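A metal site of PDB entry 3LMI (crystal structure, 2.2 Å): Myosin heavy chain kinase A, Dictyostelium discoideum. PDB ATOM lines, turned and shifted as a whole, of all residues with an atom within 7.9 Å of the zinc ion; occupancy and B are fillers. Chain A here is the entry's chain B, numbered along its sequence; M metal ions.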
ATOM      1  N   SER A 201      14.026   4.768  33.787  1.00  0.00           N
ATOM      2  CA  SER A 201      13.990   4.769  32.343  1.00  0.00           C
ATOM      3  C   SER A 201      14.264   6.142  31.722  1.00  0.00           C
ATOM      4  O   SER A 201      15.022   6.258  30.755  1.00  0.00           O
ATOM      5  CB  SER A 201      12.614   4.308  31.865  1.00  0.00           C
ATOM      6  OG  SER A 201      12.532   2.910  31.822  1.00  0.00           O
ATOM      7  N   GLN A 204      18.008   7.606  30.797  1.00  0.00           N
ATOM      8  CA  GLN A 204      18.724   6.902  29.707  1.00  0.00           C
ATOM      9  C   GLN A 204      18.084   7.138  28.323  1.00  0.00           C
ATOM     10  O   GLN A 204      18.811   7.232  27.313  1.00  0.00           O
ATOM     11  CB  GLN A 204      18.819   5.403  30.014  1.00  0.00           C
ATOM     12  CG  GLN A 204      19.225   5.080  31.479  1.00  0.00           C
ATOM     13  CD  GLN A 204      20.534   5.728  31.876  1.00  0.00           C
ATOM     14  OE1 GLN A 204      21.464   5.829  31.070  1.00  0.00           O
ATOM     15  NE2 GLN A 204      20.625   6.176  33.130  1.00  0.00           N
ATOM     16  N   ALA A 205      16.756   7.253  28.285  1.00  0.00           N
ATOM     17  CA  ALA A 205      16.014   7.531  27.044  1.00  0.00           C
ATOM     18  C   ALA A 205      16.277   8.944  26.499  1.00  0.00           C
ATOM     19  O   ALA A 205      16.395   9.147  25.282  1.00  0.00           O
ATOM     20  CB  ALA A 205      14.502   7.324  27.238  1.00  0.00           C
ATOM     21  N   PHE A 206      16.324   9.906  27.405  1.00  0.00           N
ATOM     22  CA  PHE A 206      16.736  11.253  27.048  1.00  0.00           C
ATOM     23  C   PHE A 206      18.150  11.268  26.435  1.00  0.00           C
ATOM     24  O   PHE A 206      18.379  11.914  25.401  1.00  0.00           O
ATOM     25  CB  PHE A 206      16.673  12.211  28.252  1.00  0.00           C
ATOM     26  CG  PHE A 206      17.246  13.593  27.945  1.00  0.00           C
ATOM     27  CD1 PHE A 206      16.538  14.484  27.155  1.00  0.00           C
ATOM     28  CD2 PHE A 206      18.522  13.945  28.371  1.00  0.00           C
ATOM     29  CE1 PHE A 206      17.092  15.734  26.820  1.00  0.00           C
ATOM     30  CE2 PHE A 206      19.073  15.198  28.061  1.00  0.00           C
ATOM     31  CZ  PHE A 206      18.357  16.093  27.285  1.00  0.00           C
ATOM     32  N   SER A 207      19.111  10.564  27.056  1.00  0.00           N
ATOM     33  CA  SER A 207      20.483  10.538  26.492  1.00  0.00           C
ATOM     34  C   SER A 207      20.479  10.006  25.065  1.00  0.00           C
ATOM     35  O   SER A 207      21.046  10.617  24.165  1.00  0.00           O
ATOM     36  CB  SER A 207      21.448   9.722  27.355  1.00  0.00           C
ATOM     37  OG  SER A 207      21.847  10.461  28.491  1.00  0.00           O
ATOM     38  N   HIS A 208      19.845   8.838  24.889  1.00  0.00           N
ATOM     39  CA  HIS A 208      19.695   8.219  23.579  1.00  0.00           C
ATOM     40  C   HIS A 208      19.002   9.180  22.599  1.00  0.00           C
ATOM     41  O   HIS A 208      19.502   9.421  21.480  1.00  0.00           O
ATOM     42  CB  HIS A 208      18.975   6.864  23.714  1.00  0.00           C
ATOM     43  CG  HIS A 208      18.917   6.069  22.442  1.00  0.00           C
ATOM     44  ND1 HIS A 208      18.229   4.867  22.355  1.00  0.00           N
ATOM     45  CD2 HIS A 208      19.417   6.308  21.211  1.00  0.00           C
ATOM     46  CE1 HIS A 208      18.339   4.398  21.125  1.00  0.00           C
ATOM     47  NE2 HIS A 208      19.049   5.264  20.407  1.00  0.00           N
ATOM     48  N   PHE A 209      17.889   9.781  23.033  1.00  0.00           N
ATOM     49  CA  PHE A 209      17.193  10.794  22.217  1.00  0.00           C
ATOM     50  C   PHE A 209      18.141  11.884  21.642  1.00  0.00           C
ATOM     51  O   PHE A 209      18.079  12.203  20.445  1.00  0.00           O
ATOM     52  CB  PHE A 209      16.072  11.443  23.050  1.00  0.00           C
ATOM     53  CG  PHE A 209      15.256  12.509  22.320  1.00  0.00           C
ATOM     54  CD1 PHE A 209      14.143  12.152  21.547  1.00  0.00           C
ATOM     55  CD2 PHE A 209      15.566  13.857  22.448  1.00  0.00           C
ATOM     56  CE1 PHE A 209      13.384  13.118  20.890  1.00  0.00           C
ATOM     57  CE2 PHE A 209      14.823  14.825  21.805  1.00  0.00           C
ATOM     58  CZ  PHE A 209      13.709  14.452  21.009  1.00  0.00           C
ATOM     59  N   GLU A 212      20.517  10.395  18.730  1.00  0.00           N
ATOM     60  CA  GLU A 212      19.847  10.098  17.471  1.00  0.00           C
ATOM     61  C   GLU A 212      19.383  11.373  16.771  1.00  0.00           C
ATOM     62  O   GLU A 212      19.684  11.601  15.591  1.00  0.00           O
ATOM     63  CB  GLU A 212      18.678   9.124  17.663  1.00  0.00           C
ATOM     64  CG  GLU A 212      18.099   8.636  16.340  1.00  0.00           C
ATOM     65  CD  GLU A 212      17.050   7.543  16.484  1.00  0.00           C
ATOM     66  OE1 GLU A 212      17.311   6.518  17.163  1.00  0.00           O
ATOM     67  OE2 GLU A 212      15.961   7.707  15.889  1.00  0.00           O
ATOM     68  N   PHE A 256      29.107   5.315  26.323  1.00  0.00           N
ATOM     69  CA  PHE A 256      27.639   5.330  26.453  1.00  0.00           C
ATOM     70  C   PHE A 256      26.999   4.207  25.649  1.00  0.00           C
ATOM     71  O   PHE A 256      26.137   3.489  26.156  1.00  0.00           O
ATOM     72  CB  PHE A 256      26.990   6.671  26.095  1.00  0.00           C
ATOM     73  CG  PHE A 256      25.474   6.636  26.143  1.00  0.00           C
ATOM     74  CD1 PHE A 256      24.796   6.982  27.299  1.00  0.00           C
ATOM     75  CD2 PHE A 256      24.736   6.226  25.038  1.00  0.00           C
ATOM     76  CE1 PHE A 256      23.406   6.924  27.361  1.00  0.00           C
ATOM     77  CE2 PHE A 256      23.346   6.181  25.091  1.00  0.00           C
ATOM     78  CZ  PHE A 256      22.677   6.525  26.265  1.00  0.00           C
ATOM     79  N   HIS A 260      24.334   0.976  26.891  1.00  0.00           N
ATOM     80  CA  HIS A 260      22.927   1.368  26.708  1.00  0.00           C
ATOM     81  C   HIS A 260      21.999   0.205  26.329  1.00  0.00           C
ATOM     82  O   HIS A 260      22.217  -0.463  25.316  1.00  0.00           O
ATOM     83  CB  HIS A 260      22.750   2.504  25.710  1.00  0.00           C
ATOM     84  CG  HIS A 260      21.325   2.960  25.588  1.00  0.00           C
ATOM     85  ND1 HIS A 260      20.653   3.546  26.644  1.00  0.00           N
ATOM     86  CD2 HIS A 260      20.426   2.824  24.590  1.00  0.00           C
ATOM     87  CE1 HIS A 260      19.405   3.787  26.268  1.00  0.00           C
ATOM     88  NE2 HIS A 260      19.247   3.366  25.028  1.00  0.00           N
ATOM     89  N   LYS A 261      20.938  -0.006  27.120  1.00  0.00           N
ATOM     90  CA  LYS A 261      19.889  -0.992  26.773  1.00  0.00           C
ATOM     91  C   LYS A 261      18.512  -0.319  26.650  1.00  0.00           C
ATOM     92  O   LYS A 261      18.007   0.229  27.633  1.00  0.00           O
ATOM     93  CB  LYS A 261      19.829  -2.093  27.844  1.00  0.00           C
ATOM     94  CG  LYS A 261      18.767  -3.187  27.593  1.00  0.00           C
ATOM     95  CD  LYS A 261      19.263  -4.190  26.566  1.00  0.00           C
ATOM     96  CE  LYS A 261      18.576  -5.556  26.707  1.00  0.00           C
ATOM     97  NZ  LYS A 261      17.078  -5.475  26.568  1.00  0.00           N
ATOM     98  N   CYS A 262      17.898  -0.342  25.472  1.00  0.00           N
ATOM     99  CA  CYS A 262      16.669   0.434  25.256  1.00  0.00           C
ATOM    100  C   CYS A 262      15.534  -0.003  26.202  1.00  0.00           C
ATOM    101  O   CYS A 262      15.385  -1.190  26.493  1.00  0.00           O
ATOM    102  CB  CYS A 262      16.215   0.388  23.785  1.00  0.00           C
ATOM    103  SG  CYS A 262      17.145   1.502  22.641  1.00  0.00           S
ATOM    104  N   ASN A 263      14.747   0.962  26.674  1.00  0.00           N
ATOM    105  CA  ASN A 263      13.648   0.691  27.588  1.00  0.00           C
ATOM    106  C   ASN A 263      12.307   1.116  26.987  1.00  0.00           C
ATOM    107  O   ASN A 263      12.247   1.457  25.792  1.00  0.00           O
ATOM    108  CB  ASN A 263      13.890   1.363  28.949  1.00  0.00           C
ATOM    109  CG  ASN A 263      14.153   2.862  28.837  1.00  0.00           C
ATOM    110  OD1 ASN A 263      13.322   3.616  28.326  1.00  0.00           O
ATOM    111  ND2 ASN A 263      15.304   3.306  29.355  1.00  0.00           N
ATOM    112  N   ALA A 264      11.244   1.103  27.778  1.00  0.00           N
ATOM    113  CA  ALA A 264       9.904   1.364  27.213  1.00  0.00           C
ATOM    114  C   ALA A 264       9.734   2.810  26.725  1.00  0.00           C
ATOM    115  O   ALA A 264       8.955   3.058  25.811  1.00  0.00           O
ATOM    116  CB  ALA A 264       8.801   0.988  28.219  1.00  0.00           C
ATOM    117  N   VAL A 265      10.476   3.747  27.304  1.00  0.00           N
ATOM    118  CA  VAL A 265      10.432   5.130  26.815  1.00  0.00           C
ATOM    119  C   VAL A 265      11.158   5.266  25.464  1.00  0.00           C
ATOM    120  O   VAL A 265      10.648   5.896  24.528  1.00  0.00           O
ATOM    121  CB  VAL A 265      10.968   6.121  27.866  1.00  0.00           C
ATOM    122  CG1 VAL A 265      10.959   7.554  27.321  1.00  0.00           C
ATOM    123  CG2 VAL A 265      10.119   6.032  29.125  1.00  0.00           C
ATOM    124  N   CYS A 266      12.331   4.652  25.346  1.00  0.00           N
ATOM    125  CA  CYS A 266      12.993   4.605  24.051  1.00  0.00           C
ATOM    126  C   CYS A 266      11.991   4.153  22.980  1.00  0.00           C
ATOM    127  O   CYS A 266      11.941   4.717  21.871  1.00  0.00           O
ATOM    128  CB  CYS A 266      14.203   3.655  24.079  1.00  0.00           C
ATOM    129  SG  CYS A 266      15.594   4.157  25.168  1.00  0.00           S
ATOM    130  N   ALA A 267      11.210   3.124  23.291  1.00  0.00           N
ATOM    131  CA  ALA A 267      10.257   2.556  22.341  1.00  0.00           C
ATOM    132  C   ALA A 267       9.066   3.481  22.077  1.00  0.00           C
ATOM    133  O   ALA A 267       8.673   3.673  20.938  1.00  0.00           O
ATOM    134  CB  ALA A 267       9.785   1.178  22.801  1.00  0.00           C
ATOM    135  N   LEU A 271      12.782   5.299  19.185  1.00  0.00           N
ATOM    136  CA  LEU A 271      14.221   5.312  18.960  1.00  0.00           C
ATOM    137  C   LEU A 271      14.745   4.004  18.344  1.00  0.00           C
ATOM    138  O   LEU A 271      14.154   2.938  18.527  1.00  0.00           O
ATOM    139  CB  LEU A 271      14.971   5.700  20.235  1.00  0.00           C
ATOM    140  CG  LEU A 271      14.531   7.090  20.752  1.00  0.00           C
ATOM    141  CD1 LEU A 271      15.270   7.490  22.011  1.00  0.00           C
ATOM    142  CD2 LEU A 271      14.714   8.143  19.661  1.00  0.00           C
ATOM    143  N   ASP A 272      15.855   4.111  17.631  1.00  0.00           N
ATOM    144  CA  ASP A 272      16.459   2.993  16.918  1.00  0.00           C
ATOM    145  C   ASP A 272      17.281   2.084  17.841  1.00  0.00           C
ATOM    146  O   ASP A 272      18.224   2.534  18.494  1.00  0.00           O
ATOM    147  CB  ASP A 272      17.343   3.551  15.804  1.00  0.00           C
ATOM    148  CG  ASP A 272      17.745   2.495  14.806  1.00  0.00           C
ATOM    149  OD1 ASP A 272      17.571   1.295  15.107  1.00  0.00           O
ATOM    150  OD2 ASP A 272      18.241   2.891  13.716  1.00  0.00           O
ATOM    151  N   VAL A 273      16.948   0.789  17.886  1.00  0.00           N
ATOM    152  CA  VAL A 273      17.610  -0.119  18.830  1.00  0.00           C
ATOM    153  C   VAL A 273      19.137  -0.178  18.701  1.00  0.00           C
ATOM    154  O   VAL A 273      19.837  -0.421  19.687  1.00  0.00           O
ATOM    155  CB  VAL A 273      17.049  -1.564  18.757  1.00  0.00           C
ATOM    156  CG1 VAL A 273      17.723  -2.422  19.812  1.00  0.00           C
ATOM    157  CG2 VAL A 273      15.541  -1.561  18.950  1.00  0.00           C
ATOM    158  N   LYS A 274      19.663   0.061  17.502  1.00  0.00           N
ATOM    159  CA  LYS A 274      21.102   0.068  17.299  1.00  0.00           C
ATOM    160  C   LYS A 274      21.577   1.505  17.134  1.00  0.00           C
ATOM    161  O   LYS A 274      21.026   2.252  16.320  1.00  0.00           O
ATOM    162  CB  LYS A 274      21.481  -0.754  16.069  1.00  0.00           C
ATOM    163  CG  LYS A 274      21.055  -2.224  16.140  1.00  0.00           C
ATOM    164  CD  LYS A 274      21.753  -3.058  15.056  1.00  0.00           C
ATOM    165  CE  LYS A 274      21.857  -4.538  15.461  1.00  0.00           C
ATOM    166  NZ  LYS A 274      22.570  -4.732  16.758  1.00  0.00           N
ATOM    167  N   LEU A 275      22.589   1.893  17.903  1.00  0.00           N
ATOM    168  CA  LEU A 275      23.086   3.260  17.821  1.00  0.00           C
ATOM    169  C   LEU A 275      24.224   3.387  16.806  1.00  0.00           C
ATOM    170  O   LEU A 275      24.691   4.492  16.520  1.00  0.00           O
ATOM    171  CB  LEU A 275      23.548   3.758  19.190  1.00  0.00           C
ATOM    172  CG  LEU A 275      22.820   3.242  20.435  1.00  0.00           C
ATOM    173  CD1 LEU A 275      22.729   4.355  21.445  1.00  0.00           C
ATOM    174  CD2 LEU A 275      21.437   2.680  20.105  1.00  0.00           C
HETATM  175 ZN    ZN M   1      17.468   3.583  23.890  1.00  0.00          ZN
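NE2 of His 260 is bound to the zinc ion, at 2.1 Å. ND1 of His 208 is bound to the zinc ion (2.1 Å). SG of Cys 266 is bound to the zinc ion (2.3 Å). SG of Cys 262 binds the zinc ion, 2.4 Å away. The zinc ion has four donor atoms within binding distance.
NE2 of His 208 lies close to O of Asp 272, 3.4 Å away. N of Leu 271 sits at hydrogen-bond distance from O of Cys 266, 2.9 Å away. N of Cys 266 sits at hydrogen-bond distance from OD1 of Asn 263 (3.3 Å).
Along chain A the residues within 4 Å of the zinc ion span positions 208 to 266. The nearest printed residue that does not touch the zinc ion is Asn 263 (4.7 Å).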
